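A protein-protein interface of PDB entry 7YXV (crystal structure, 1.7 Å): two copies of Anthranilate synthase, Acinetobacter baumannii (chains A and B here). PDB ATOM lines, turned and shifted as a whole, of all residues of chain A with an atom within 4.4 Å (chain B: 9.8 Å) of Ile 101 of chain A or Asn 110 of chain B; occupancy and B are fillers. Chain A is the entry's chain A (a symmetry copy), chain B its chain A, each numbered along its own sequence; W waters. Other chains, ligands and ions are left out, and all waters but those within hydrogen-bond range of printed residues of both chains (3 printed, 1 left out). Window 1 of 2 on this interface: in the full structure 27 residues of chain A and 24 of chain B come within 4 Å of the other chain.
OD1 of Asn 110 of chain B is in hydrogen-bond range of NZ of Lys 77 of chain A, 2.8 Å away. NE2 of Gln 3 of chain B is in hydrogen-bond range of OE2 of Glu 100 of chain A. The side-chain amide nitrogen (ND2) of Asn 110 of chain B sits at hydrogen-bond distance from the side-chain carboxylate (OE1) of Glu 105 of chain A (3.0 Å). O of Asn 110 of chain B sits at hydrogen-bond distance from N of Ile 103 of chain A, at 2.8 Å. The backbone carbonyl oxygen (O) of Ile 101 of chain A is in hydrogen-bond range of the backbone NH (N) of Gly 112 of chain B, 2.9 Å away.
NZ of Lys 77 of chain A is in salt-bridge range of OE2 of Glu 105 of chain A, 3.0 Å away. The backbone NH of Ile 64 of chain A lies within hydrogen-bond range of the backbone carbonyl oxygen of Glu 100 of chain A (2.8 Å). N of Gln 3 of chain B lies within hydrogen-bond range of O of Ser 67 of chain B. O of Ile 64 of chain A sits at hydrogen-bond distance from N of Thr 102 of chain A (2.9 Å).
Among the printed residues, pairs that only touch across the chains: Ile 81 of chain A with Glu 109 of chain B (3.7 Å), Ile 81 of chain A with Asn 110 of chain B (3.5 Å), Ile 81 of chain A with Trp 111 of chain B (3.9 Å), Ile 81 of chain A with Gly 112 of chain B (3.8 Å), Ile 81 of chain A with Asn 117 of chain B (3.7 Å), Phe 85 of chain A with Gly 112 of chain B (3.6 Å), Phe 85 of chain A with Ile 113 of chain B (3.8 Å), Phe 85 of chain A with Gly 115 of chain B (3.4 Å), Phe 85 of chain A with Lys 116 of chain B (3.8 Å), Ile 99 of chain A with Arg 114 of chain B (3.8 Å), Glu 100 of chain A with Met 1 of chain B (3.3 Å), Glu 100 of chain A with Trp 111 of chain B (3.4 Å), Glu 100 of chain A with Gly 112 of chain B (3.3 Å), Ile 101 of chain A with Asn 110 of chain B (3.8 Å), Ile 101 of chain A with Trp 111 of chain B (3.2 Å), Thr 102 of chain A with Thr 106 of chain B (3.9 Å), Thr 102 of chain A with Asn 110 of chain B (3.4 Å), Thr 102 of chain A with Trp 111 of chain B (3.3 Å) and Ile 103 of chain A with Thr 106 of chain B (3.5 Å).
No residue of chain B comes within 4 Å of Ile 64 of chain A. Of the printed residues of chain B, Phe 85 of chain A touches Gly 112, Ile 113, Gly 115 and Lys 116. Glu 100 of chain A touches just these residues of chain B: Met 1 (3.3 Å), Gln 3 (2.8 Å), Trp 111 (3.4 Å) and Gly 112 (3.3 Å). Ile 101 of chain A touches just these residues of chain B: Asn 110, Trp 111 and Gly 112. Thr 102 of chain A touches just these residues of chain B: Thr 106 (3.9 Å), Asn 110 (3.4 Å) and Trp 111 (3.3 Å). Of chain B, only Thr 106 (3.5 Å) and Asn 110 (2.8 Å) come within 4 Å of Ile 103 of chain A. Of the printed residues of chain A, Thr 106 of chain B touches Thr 102 (3.9 Å) and Ile 103 (3.5 Å). Of the printed residues of chain A, Asn 110 of chain B touches Lys 77, Ile 81, Ile 101, Thr 102, Ile 103 and Glu 105. Of the printed residues of chain A, Gly 112 of chain B touches Ile 81 (3.8 Å), Phe 85 (3.6 Å), Glu 100 (3.3 Å) and Ile 101 (2.9 Å). The nearest residue of chain B that does not touch Ile 101 of chain A is Ile 113 of chain B (5.2 Å). The nearest printed residue of chain B that does not touch Ile 81 of chain A is Lys 116 of chain B (5.0 Å).
Of the 23 printed residues of chain B, 12 touch a printed residue of chain A. Printed residues of chain B that touch a printed residue of chain A: Met 1, Gln 3, Thr 106, Glu 109, Asn 110, Trp 111, Gly 112, Ile 113, Arg 114, Gly 115, Lys 116 and Asn 117. Hydrophobic or aromatic side chains of chain B within 4 Å of the printed part of chain A: Met 1 and Trp 111. Printed residues of chain A that touch a printed residue of chain B: Lys 77, Ile 81, Phe 85, Ile 99, Glu 100, Ile 101, Thr 102, Ile 103 and Glu 105. Hydrophobic or aromatic side chains of chain A that line the printed part of chain B: Ile 81, Phe 85 and Ile 103.
1 position is printed for both chains. Of the 24 pairs that touch across the chains among the printed residues, none has its exchanged pair printed and touching as well.
Water W2 lies within hydrogen-bond range of OE2 of Glu 109 of chain B (2.5 Å) and NZ of Lys 77 of chain A (2.9 Å). Water W1 lies within hydrogen-bond range of the side-chain hydroxyl of Ser 67 of chain B and the side-chain hydroxyl of Thr 102 of chain A. Water W3 lies within hydrogen-bond range of O of Ile 99 of chain A and N of Arg 114 of chain B.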
ATOM      1  N   ILE A  64      -1.173  -3.622  -6.326  1.00  0.00           N
ATOM      2  CA  ILE A  64      -2.594  -3.923  -6.437  1.00  0.00           C
ATOM      3  C   ILE A  64      -3.271  -2.638  -6.934  1.00  0.00           C
ATOM      4  O   ILE A  64      -3.240  -1.669  -6.213  1.00  0.00           O
ATOM      5  CB  ILE A  64      -3.165  -4.433  -5.084  1.00  0.00           C
ATOM      6  CG1 ILE A  64      -2.414  -5.676  -4.629  1.00  0.00           C
ATOM      7  CG2 ILE A  64      -4.655  -4.692  -5.210  1.00  0.00           C
ATOM      8  CD1 ILE A  64      -2.647  -6.053  -3.181  1.00  0.00           C
ATOM      9  N   LEU A  66      -7.000  -1.253  -7.797  1.00  0.00           N
ATOM     10  CA  LEU A  66      -8.439  -1.566  -7.571  1.00  0.00           C
ATOM     11  C   LEU A  66      -9.212  -0.458  -8.297  1.00  0.00           C
ATOM     12  O   LEU A  66      -9.133   0.677  -7.899  1.00  0.00           O
ATOM     13  CB  LEU A  66      -8.803  -1.531  -6.101  1.00  0.00           C
ATOM     14  CG  LEU A  66      -8.333  -2.613  -5.160  1.00  0.00           C
ATOM     15  CD1 LEU A  66      -7.071  -2.149  -4.501  1.00  0.00           C
ATOM     16  CD2 LEU A  66      -9.429  -2.871  -4.119  1.00  0.00           C
ATOM     17  N   LYS A  77     -11.827   4.888   2.094  1.00  0.00           N
ATOM     18  CA  LYS A  77     -10.813   4.341   1.210  1.00  0.00           C
ATOM     19  C   LYS A  77      -9.533   4.003   1.968  1.00  0.00           C
ATOM     20  O   LYS A  77      -8.933   2.955   1.780  1.00  0.00           O
ATOM     21  CB  LYS A  77     -10.541   5.277   0.036  1.00  0.00           C
ATOM     22  CG  LYS A  77     -11.602   5.247  -1.015  1.00  0.00           C
ATOM     23  CD  LYS A  77     -11.316   6.241  -2.059  1.00  0.00           C
ATOM     24  CE  LYS A  77     -11.421   7.689  -1.681  1.00  0.00           C
ATOM     25  NZ  LYS A  77     -11.186   8.483  -2.901  1.00  0.00           N
ATOM     26  N   ILE A  81      -7.705   0.261   2.447  1.00  0.00           N
ATOM     27  CA  ILE A  81      -6.313   0.030   2.193  1.00  0.00           C
ATOM     28  C   ILE A  81      -5.631  -0.615   3.380  1.00  0.00           C
ATOM     29  O   ILE A  81      -4.844  -1.515   3.220  1.00  0.00           O
ATOM     30  CB  ILE A  81      -5.602   1.317   1.749  1.00  0.00           C
ATOM     31  CG1 ILE A  81      -6.065   1.566   0.279  1.00  0.00           C
ATOM     32  CG2 ILE A  81      -4.079   1.283   1.942  1.00  0.00           C
ATOM     33  CD1 ILE A  81      -5.814   2.956  -0.258  1.00  0.00           C
ATOM     34  N   LEU A  84      -6.553  -4.279   3.472  1.00  0.00           N
ATOM     35  CA  LEU A  84      -5.819  -5.059   2.528  1.00  0.00           C
ATOM     36  C   LEU A  84      -4.389  -5.373   3.026  1.00  0.00           C
ATOM     37  O   LEU A  84      -3.958  -6.513   2.935  1.00  0.00           O
ATOM     38  CB  LEU A  84      -5.699  -4.242   1.233  1.00  0.00           C
ATOM     39  CG  LEU A  84      -6.966  -4.261   0.391  1.00  0.00           C
ATOM     40  CD1 LEU A  84      -7.058  -3.147  -0.683  1.00  0.00           C
ATOM     41  CD2 LEU A  84      -7.134  -5.605  -0.295  1.00  0.00           C
ATOM     42  N   PHE A  85      -3.686  -4.356   3.555  1.00  0.00           N
ATOM     43  CA  PHE A  85      -2.426  -4.569   4.152  1.00  0.00           C
ATOM     44  C   PHE A  85      -2.482  -5.682   5.213  1.00  0.00           C
ATOM     45  O   PHE A  85      -1.614  -6.563   5.246  1.00  0.00           O
ATOM     46  CB  PHE A  85      -1.849  -3.288   4.797  1.00  0.00           C
ATOM     47  CG  PHE A  85      -1.273  -2.277   3.820  1.00  0.00           C
ATOM     48  CD1 PHE A  85      -0.286  -2.658   2.871  1.00  0.00           C
ATOM     49  CD2 PHE A  85      -1.668  -0.935   3.865  1.00  0.00           C
ATOM     50  CE1 PHE A  85       0.286  -1.706   1.998  1.00  0.00           C
ATOM     51  CE2 PHE A  85      -1.081   0.006   3.034  1.00  0.00           C
ATOM     52  CZ  PHE A  85      -0.096  -0.383   2.093  1.00  0.00           C
ATOM     53  N   ILE A  99       4.044  -4.321  -0.189  1.00  0.00           N
ATOM     54  CA  ILE A  99       2.702  -4.258  -0.780  1.00  0.00           C
ATOM     55  C   ILE A  99       2.425  -2.808  -1.144  1.00  0.00           C
ATOM     56  O   ILE A  99       2.565  -1.904  -0.316  1.00  0.00           O
ATOM     57  CB  ILE A  99       1.609  -4.832   0.167  1.00  0.00           C
ATOM     58  CG1 ILE A  99       1.778  -6.372   0.428  1.00  0.00           C
ATOM     59  CG2 ILE A  99       0.217  -4.478  -0.355  1.00  0.00           C
ATOM     60  CD1 ILE A  99       2.031  -7.239  -0.806  1.00  0.00           C
ATOM     61  N   GLU A 100       1.938  -2.595  -2.371  1.00  0.00           N
ATOM     62  CA  GLU A 100       1.513  -1.272  -2.779  1.00  0.00           C
ATOM     63  C   GLU A 100       0.151  -1.317  -3.433  1.00  0.00           C
ATOM     64  O   GLU A 100      -0.140  -2.270  -4.122  1.00  0.00           O
ATOM     65  CB  GLU A 100       2.562  -0.663  -3.745  1.00  0.00           C
ATOM     66  CG  GLU A 100       2.244   0.743  -4.079  1.00  0.00           C
ATOM     67  CD  GLU A 100       3.284   1.421  -4.921  1.00  0.00           C
ATOM     68  OE1 GLU A 100       4.512   1.197  -4.717  1.00  0.00           O
ATOM     69  OE2 GLU A 100       2.846   2.152  -5.868  1.00  0.00           O
ATOM     70  N   ILE A 101      -0.668  -0.308  -3.125  1.00  0.00           N
ATOM     71  CA  ILE A 101      -2.064  -0.309  -3.523  1.00  0.00           C
ATOM     72  C   ILE A 101      -2.382   1.051  -4.130  1.00  0.00           C
ATOM     73  O   ILE A 101      -2.048   2.085  -3.567  1.00  0.00           O
ATOM     74  CB  ILE A 101      -2.989  -0.602  -2.347  1.00  0.00           C
ATOM     75  CG1 ILE A 101      -2.663  -1.965  -1.748  1.00  0.00           C
ATOM     76  CG2 ILE A 101      -4.450  -0.438  -2.795  1.00  0.00           C
ATOM     77  CD1 ILE A 101      -3.099  -2.100  -0.295  1.00  0.00           C
ATOM     78  N   THR A 102      -3.111   1.077  -5.254  1.00  0.00           N
ATOM     79  CA  THR A 102      -3.729   2.275  -5.721  1.00  0.00           C
ATOM     80  C   THR A 102      -5.161   1.992  -6.140  1.00  0.00           C
ATOM     81  O   THR A 102      -5.454   1.059  -6.907  1.00  0.00           O
ATOM     82  CB  THR A 102      -2.997   2.951  -6.934  1.00  0.00           C
ATOM     83  OG1 THR A 102      -1.601   3.110  -6.634  1.00  0.00           O
ATOM     84  CG2 THR A 102      -3.693   4.290  -7.285  1.00  0.00           C
ATOM     85  N   ILE A 103      -6.056   2.826  -5.627  1.00  0.00           N
ATOM     86  CA  ILE A 103      -7.502   2.822  -6.021  1.00  0.00           C
ATOM     87  C   ILE A 103      -7.723   3.838  -7.120  1.00  0.00           C
ATOM     88  O   ILE A 103      -7.264   4.987  -7.050  1.00  0.00           O
ATOM     89  CB  ILE A 103      -8.388   3.213  -4.828  1.00  0.00           C
ATOM     90  CG1 ILE A 103      -8.303   2.161  -3.744  1.00  0.00           C
ATOM     91  CG2 ILE A 103      -9.835   3.480  -5.211  1.00  0.00           C
ATOM     92  CD1 ILE A 103      -8.920   2.595  -2.373  1.00  0.00           C
ATOM     93  N   GLU A 105     -10.930   5.497  -9.501  1.00  0.00           N
ATOM     94  CA  GLU A 105     -12.387   5.712  -9.344  1.00  0.00           C
ATOM     95  C   GLU A 105     -12.944   6.310 -10.621  1.00  0.00           C
ATOM     96  O   GLU A 105     -12.270   7.205 -11.236  1.00  0.00           O
ATOM     97  CB  GLU A 105     -12.646   6.722  -8.226  1.00  0.00           C
ATOM     98  CG  GLU A 105     -12.268   6.223  -6.832  1.00  0.00           C
ATOM     99  CD  GLU A 105     -12.173   7.344  -5.809  1.00  0.00           C
ATOM    100  OE1 GLU A 105     -11.244   8.163  -5.935  1.00  0.00           O
ATOM    101  OE2 GLU A 105     -13.099   7.372  -4.998  1.00  0.00           O
ATOM    102  N   MET B   1       5.116  10.464  -5.880  1.00  0.00           N
ATOM    103  CA  MET B   1       5.144   9.030  -6.290  1.00  0.00           C
ATOM    104  C   MET B   1       4.692   8.935  -7.700  1.00  0.00           C
ATOM    105  O   MET B   1       3.690   9.598  -8.053  1.00  0.00           O
ATOM    106  CB  MET B   1       4.176   8.170  -5.465  1.00  0.00           C
ATOM    107  CG  MET B   1       4.315   6.679  -5.740  1.00  0.00           C
ATOM    108  SD  MET B   1       5.928   5.988  -5.205  1.00  0.00           S
ATOM    109  CE  MET B   1       5.573   4.249  -5.462  1.00  0.00           C
ATOM    110  N   GLN B   3       4.082   5.825 -10.634  1.00  0.00           N
ATOM    111  CA  GLN B   3       4.167   4.437 -11.078  1.00  0.00           C
ATOM    112  C   GLN B   3       4.121   4.446 -12.601  1.00  0.00           C
ATOM    113  O   GLN B   3       3.104   4.938 -13.155  1.00  0.00           O
ATOM    114  CB  GLN B   3       2.975   3.633 -10.594  1.00  0.00           C
ATOM    115  CG  GLN B   3       3.190   3.041  -9.184  1.00  0.00           C
ATOM    116  CD  GLN B   3       4.272   1.984  -9.144  1.00  0.00           C
ATOM    117  OE1 GLN B   3       4.681   1.495 -10.178  1.00  0.00           O
ATOM    118  NE2 GLN B   3       4.717   1.600  -7.919  1.00  0.00           N
ATOM    119  N   ARG B  42       7.119  -0.829 -14.892  1.00  0.00           N
ATOM    120  CA  ARG B  42       6.709  -2.118 -15.352  1.00  0.00           C
ATOM    121  C   ARG B  42       6.698  -2.038 -16.910  1.00  0.00           C
ATOM    122  O   ARG B  42       5.982  -1.220 -17.478  1.00  0.00           O
ATOM    123  CB  ARG B  42       5.306  -2.435 -14.878  1.00  0.00           C
ATOM    124  CG  ARG B  42       5.266  -2.947 -13.434  1.00  0.00           C
ATOM    125  CD  ARG B  42       3.893  -2.878 -12.799  1.00  0.00           C
ATOM    126  NE  ARG B  42       3.601  -1.464 -12.482  1.00  0.00           N
ATOM    127  CZ  ARG B  42       2.445  -1.000 -12.081  1.00  0.00           C
ATOM    128  NH1 ARG B  42       1.377  -1.773 -12.005  1.00  0.00           N
ATOM    129  NH2 ARG B  42       2.319   0.257 -11.758  1.00  0.00           N
ATOM    130  N   SER B  67       1.148   6.903 -13.530  1.00  0.00           N
ATOM    131  CA  SER B  67       0.157   7.126 -12.508  1.00  0.00           C
ATOM    132  C   SER B  67       0.790   7.893 -11.309  1.00  0.00           C
ATOM    133  O   SER B  67       1.803   7.437 -10.794  1.00  0.00           O
ATOM    134  CB  SER B  67      -0.331   5.793 -12.045  1.00  0.00           C
ATOM    135  OG  SER B  67      -1.249   5.894 -10.977  1.00  0.00           O
ATOM    136  N   MET B  68       0.256   9.065 -11.031  1.00  0.00           N
ATOM    137  CA  MET B  68       0.884  10.007 -10.095  1.00  0.00           C
ATOM    138  C   MET B  68      -0.195  10.546  -9.160  1.00  0.00           C
ATOM    139  O   MET B  68      -1.393  10.419  -9.421  1.00  0.00           O
ATOM    140  CB  MET B  68       1.668  11.105 -10.758  1.00  0.00           C
ATOM    141  CG  MET B  68       0.862  12.061 -11.549  1.00  0.00           C
ATOM    142  SD  MET B  68       2.092  13.172 -12.310  1.00  0.00           S
ATOM    143  CE  MET B  68       2.712  12.136 -13.581  1.00  0.00           C
ATOM    144  N   PHE B  69       0.274  11.229  -8.132  1.00  0.00           N
ATOM    145  CA  PHE B  69      -0.674  11.938  -7.275  1.00  0.00           C
ATOM    146  C   PHE B  69      -1.254  13.162  -7.997  1.00  0.00           C
ATOM    147  O   PHE B  69      -0.548  13.823  -8.787  1.00  0.00           O
ATOM    148  CB  PHE B  69      -0.013  12.428  -5.968  1.00  0.00           C
ATOM    149  CG  PHE B  69       0.606  11.355  -5.111  1.00  0.00           C
ATOM    150  CD1 PHE B  69       0.026  10.158  -4.918  1.00  0.00           C
ATOM    151  CD2 PHE B  69       1.703  11.669  -4.312  1.00  0.00           C
ATOM    152  CE1 PHE B  69       0.581   9.209  -4.084  1.00  0.00           C
ATOM    153  CE2 PHE B  69       2.262  10.769  -3.415  1.00  0.00           C
ATOM    154  CZ  PHE B  69       1.699   9.500  -3.300  1.00  0.00           C
ATOM    155  N   ALA B  70      -2.513  13.430  -7.706  1.00  0.00           N
ATOM    156  CA  ALA B  70      -3.193  14.601  -8.158  1.00  0.00           C
ATOM    157  C   ALA B  70      -2.522  15.879  -7.649  1.00  0.00           C
ATOM    158  O   ALA B  70      -1.783  15.883  -6.661  1.00  0.00           O
ATOM    159  CB  ALA B  70      -4.651  14.565  -7.704  1.00  0.00           C
ATOM    160  N   GLU B 105      -4.063  10.511 -12.656  1.00  0.00           N
ATOM    161  CA  GLU B 105      -3.909  11.204 -11.357  1.00  0.00           C
ATOM    162  C   GLU B 105      -4.960  10.694 -10.390  1.00  0.00           C
ATOM    163  O   GLU B 105      -6.146  10.477 -10.817  1.00  0.00           O
ATOM    164  CB  GLU B 105      -4.153  12.703 -11.534  1.00  0.00           C
ATOM    165  CG  GLU B 105      -3.095  13.414 -12.376  1.00  0.00           C
ATOM    166  CD  GLU B 105      -3.543  14.787 -12.852  1.00  0.00           C
ATOM    167  OE1 GLU B 105      -4.463  14.835 -13.691  1.00  0.00           O
ATOM    168  OE2 GLU B 105      -2.994  15.727 -12.278  1.00  0.00           O
ATOM    169  N   THR B 106      -4.532  10.534  -9.127  1.00  0.00           N
ATOM    170  CA  THR B 106      -5.455  10.062  -8.056  1.00  0.00           C
ATOM    171  C   THR B 106      -5.025  10.799  -6.788  1.00  0.00           C
ATOM    172  O   THR B 106      -3.882  11.177  -6.652  1.00  0.00           O
ATOM    173  CB  THR B 106      -5.360   8.534  -7.792  1.00  0.00           C
ATOM    174  OG1 THR B 106      -3.973   8.161  -7.771  1.00  0.00           O
ATOM    175  CG2 THR B 106      -6.170   7.784  -8.788  1.00  0.00           C
ATOM    176  N   PRO B 107      -5.963  11.013  -5.875  1.00  0.00           N
ATOM    177  CA  PRO B 107      -5.546  11.620  -4.629  1.00  0.00           C
ATOM    178  C   PRO B 107      -4.703  10.683  -3.762  1.00  0.00           C
ATOM    179  O   PRO B 107      -4.807   9.457  -3.852  1.00  0.00           O
ATOM    180  CB  PRO B 107      -6.849  11.943  -3.943  1.00  0.00           C
ATOM    181  CG  PRO B 107      -7.876  11.128  -4.602  1.00  0.00           C
ATOM    182  CD  PRO B 107      -7.368  10.645  -5.910  1.00  0.00           C
ATOM    183  N   LYS B 108      -3.928  11.271  -2.871  1.00  0.00           N
ATOM    184  CA  LYS B 108      -3.016  10.473  -2.001  1.00  0.00           C
ATOM    185  C   LYS B 108      -3.722   9.419  -1.150  1.00  0.00           C
ATOM    186  O   LYS B 108      -3.188   8.362  -0.900  1.00  0.00           O
ATOM    187  CB  LYS B 108      -2.161  11.379  -1.105  1.00  0.00           C
ATOM    188  CG  LYS B 108      -1.219  12.247  -1.916  1.00  0.00           C
ATOM    189  CD  LYS B 108      -0.450  13.213  -1.006  1.00  0.00           C
ATOM    190  CE  LYS B 108       0.747  13.822  -1.725  1.00  0.00           C
ATOM    191  NZ  LYS B 108       1.241  14.918  -0.850  1.00  0.00           N
ATOM    192  N   GLU B 109      -4.951   9.726  -0.758  1.00  0.00           N
ATOM    193  CA  GLU B 109      -5.747   8.828   0.106  1.00  0.00           C
ATOM    194  C   GLU B 109      -6.128   7.535  -0.643  1.00  0.00           C
ATOM    195  O   GLU B 109      -6.497   6.584  -0.019  1.00  0.00           O
ATOM    196  CB  GLU B 109      -7.046   9.448   0.654  1.00  0.00           C
ATOM    197  CG  GLU B 109      -8.057   9.951  -0.381  1.00  0.00           C
ATOM    198  CD  GLU B 109      -7.956  11.444  -0.673  1.00  0.00           C
ATOM    199  OE1 GLU B 109      -6.837  11.907  -0.615  1.00  0.00           O
ATOM    200  OE2 GLU B 109      -8.991  12.151  -1.007  1.00  0.00           O
ATOM    201  N   ASN B 110      -5.983   7.516  -1.963  1.00  0.00           N
ATOM    202  CA  ASN B 110      -6.145   6.340  -2.757  1.00  0.00           C
ATOM    203  C   ASN B 110      -4.969   5.383  -2.823  1.00  0.00           C
ATOM    204  O   ASN B 110      -5.082   4.304  -3.419  1.00  0.00           O
ATOM    205  CB  ASN B 110      -6.521   6.711  -4.190  1.00  0.00           C
ATOM    206  CG  ASN B 110      -7.936   7.205  -4.330  1.00  0.00           C
ATOM    207  OD1 ASN B 110      -8.477   7.804  -3.421  1.00  0.00           O
ATOM    208  ND2 ASN B 110      -8.520   7.030  -5.541  1.00  0.00           N
ATOM    209  N   TRP B 111      -3.876   5.705  -2.139  1.00  0.00           N
ATOM    210  CA  TRP B 111      -2.657   4.914  -2.194  1.00  0.00           C
ATOM    211  C   TRP B 111      -2.253   4.364  -0.842  1.00  0.00           C
ATOM    212  O   TRP B 111      -2.257   5.092   0.183  1.00  0.00           O
ATOM    213  CB  TRP B 111      -1.517   5.792  -2.713  1.00  0.00           C
ATOM    214  CG  TRP B 111      -1.569   6.251  -4.104  1.00  0.00           C
ATOM    215  CD1 TRP B 111      -2.414   7.184  -4.582  1.00  0.00           C
ATOM    216  CD2 TRP B 111      -0.629   5.973  -5.151  1.00  0.00           C
ATOM    217  NE1 TRP B 111      -2.119   7.466  -5.901  1.00  0.00           N
ATOM    218  CE2 TRP B 111      -1.030   6.733  -6.273  1.00  0.00           C
ATOM    219  CE3 TRP B 111       0.524   5.161  -5.265  1.00  0.00           C
ATOM    220  CZ2 TRP B 111      -0.378   6.670  -7.483  1.00  0.00           C
ATOM    221  CZ3 TRP B 111       1.175   5.096  -6.511  1.00  0.00           C
ATOM    222  CH2 TRP B 111       0.736   5.890  -7.575  1.00  0.00           C
ATOM    223  N   GLY B 112      -1.772   3.111  -0.918  1.00  0.00           N
ATOM    224  CA  GLY B 112      -1.003   2.493   0.145  1.00  0.00           C
ATOM    225  C   GLY B 112       0.413   2.259  -0.275  1.00  0.00           C
ATOM    226  O   GLY B 112       0.610   1.571  -1.259  1.00  0.00           O
ATOM    227  N   ILE B 113       1.389   2.755   0.506  1.00  0.00           N
ATOM    228  CA  ILE B 113       2.793   2.571   0.214  1.00  0.00           C
ATOM    229  C   ILE B 113       3.515   2.121   1.480  1.00  0.00           C
ATOM    230  O   ILE B 113       3.340   2.767   2.483  1.00  0.00           O
ATOM    231  CB  ILE B 113       3.351   3.920  -0.318  1.00  0.00           C
ATOM    232  CG1 ILE B 113       2.647   4.353  -1.557  1.00  0.00           C
ATOM    233  CG2 ILE B 113       4.878   3.882  -0.457  1.00  0.00           C
ATOM    234  CD1 ILE B 113       2.885   5.783  -1.994  1.00  0.00           C
ATOM    235  N   ARG B 114       4.237   1.003   1.412  1.00  0.00           N
ATOM    236  CA  ARG B 114       5.043   0.486   2.539  1.00  0.00           C
ATOM    237  C   ARG B 114       4.192   0.368   3.809  1.00  0.00           C
ATOM    238  O   ARG B 114       4.623   0.646   4.900  1.00  0.00           O
ATOM    239  CB  ARG B 114       6.318   1.336   2.690  1.00  0.00           C
ATOM    240  CG  ARG B 114       7.240   1.252   1.437  1.00  0.00           C
ATOM    241  CD  ARG B 114       8.515   2.125   1.515  1.00  0.00           C
ATOM    242  NE  ARG B 114       8.231   3.555   1.607  1.00  0.00           N
ATOM    243  CZ  ARG B 114       9.136   4.541   1.718  1.00  0.00           C
ATOM    244  NH1 ARG B 114       8.712   5.780   1.768  1.00  0.00           N
ATOM    245  NH2 ARG B 114      10.448   4.316   1.722  1.00  0.00           N
ATOM    246  N   GLY B 115       2.938  -0.059   3.649  1.00  0.00           N
ATOM    247  CA  GLY B 115       2.027  -0.247   4.770  1.00  0.00           C
ATOM    248  C   GLY B 115       1.349   0.986   5.313  1.00  0.00           C
ATOM    249  O   GLY B 115       0.622   0.897   6.308  1.00  0.00           O
ATOM    250  N   LYS B 116       1.562   2.114   4.666  1.00  0.00           N
ATOM    251  CA  LYS B 116       1.030   3.374   5.100  1.00  0.00           C
ATOM    252  C   LYS B 116       0.032   3.907   4.093  1.00  0.00           C
ATOM    253  O   LYS B 116       0.197   3.777   2.865  1.00  0.00           O
ATOM    254  CB  LYS B 116       2.091   4.405   5.291  1.00  0.00           C
ATOM    255  CG  LYS B 116       2.987   3.977   6.482  1.00  0.00           C
ATOM    256  CD  LYS B 116       4.098   4.939   6.810  1.00  0.00           C
ATOM    257  CE  LYS B 116       5.071   4.267   7.800  1.00  0.00           C
ATOM    258  NZ  LYS B 116       5.756   5.250   8.684  1.00  0.00           N
ATOM    259  N   ASN B 117      -0.949   4.627   4.607  1.00  0.00           N
ATOM    260  CA  ASN B 117      -1.791   5.493   3.766  1.00  0.00           C
ATOM    261  C   ASN B 117      -0.971   6.668   3.278  1.00  0.00           C
ATOM    262  O   ASN B 117      -0.354   7.396   4.076  1.00  0.00           O
ATOM    263  CB  ASN B 117      -3.014   5.954   4.531  1.00  0.00           C
ATOM    264  CG  ASN B 117      -3.890   4.806   5.015  1.00  0.00           C
ATOM    265  OD1 ASN B 117      -3.847   4.434   6.203  1.00  0.00           O
ATOM    266  ND2 ASN B 117      -4.624   4.192   4.122  1.00  0.00           N
ATOM    267  N   ALA B 118      -0.907   6.920   1.958  1.00  0.00           N
ATOM    268  CA  ALA B 118       0.009   7.886   1.460  1.00  0.00           C
ATOM    269  C   ALA B 118      -0.215   9.331   1.951  1.00  0.00           C
ATOM    270  O   ALA B 118       0.726  10.126   2.028  1.00  0.00           O
ATOM    271  CB  ALA B 118       0.079   7.876  -0.057  1.00  0.00           C
ATOM    272  N   ASP B 119      -1.439   9.696   2.292  1.00  0.00           N
ATOM    273  CA  ASP B 119      -1.720  11.004   2.789  1.00  0.00           C
ATOM    274  C   ASP B 119      -1.029  11.225   4.144  1.00  0.00           C
ATOM    275  O   ASP B 119      -0.842  12.401   4.514  1.00  0.00           O
ATOM    276  CB  ASP B 119      -3.258  11.229   2.900  1.00  0.00           C
ATOM    277  CG  ASP B 119      -3.861  10.351   3.943  1.00  0.00           C
ATOM    278  OD1 ASP B 119      -3.742   9.111   3.759  1.00  0.00           O
ATOM    279  OD2 ASP B 119      -4.475  10.883   4.911  1.00  0.00           O
ATOM    280  N   GLU B 120      -0.685  10.184   4.846  1.00  0.00           N
ATOM    281  CA  GLU B 120      -0.177  10.318   6.215  1.00  0.00           C
ATOM    282  C   GLU B 120       1.339  10.534   6.293  1.00  0.00           C
ATOM    283  O   GLU B 120       1.858  10.830   7.367  1.00  0.00           O
ATOM    284  CB  GLU B 120      -0.543   9.099   7.008  1.00  0.00           C
ATOM    285  CG  GLU B 120      -2.062   8.984   7.261  1.00  0.00           C
ATOM    286  CD  GLU B 120      -2.465   7.800   8.118  1.00  0.00           C
ATOM    287  OE1 GLU B 120      -1.593   7.008   8.649  1.00  0.00           O
ATOM    288  OE2 GLU B 120      -3.667   7.595   8.287  1.00  0.00           O
HETATM  289  O   HOH W   1      -0.841   3.717  -9.512  1.00  0.00           O
HETATM  290  O   HOH W   2     -11.181  11.151  -1.755  1.00  0.00           O
HETATM  291  O   HOH W   3       5.138  -0.957  -0.513  1.00  0.00           O
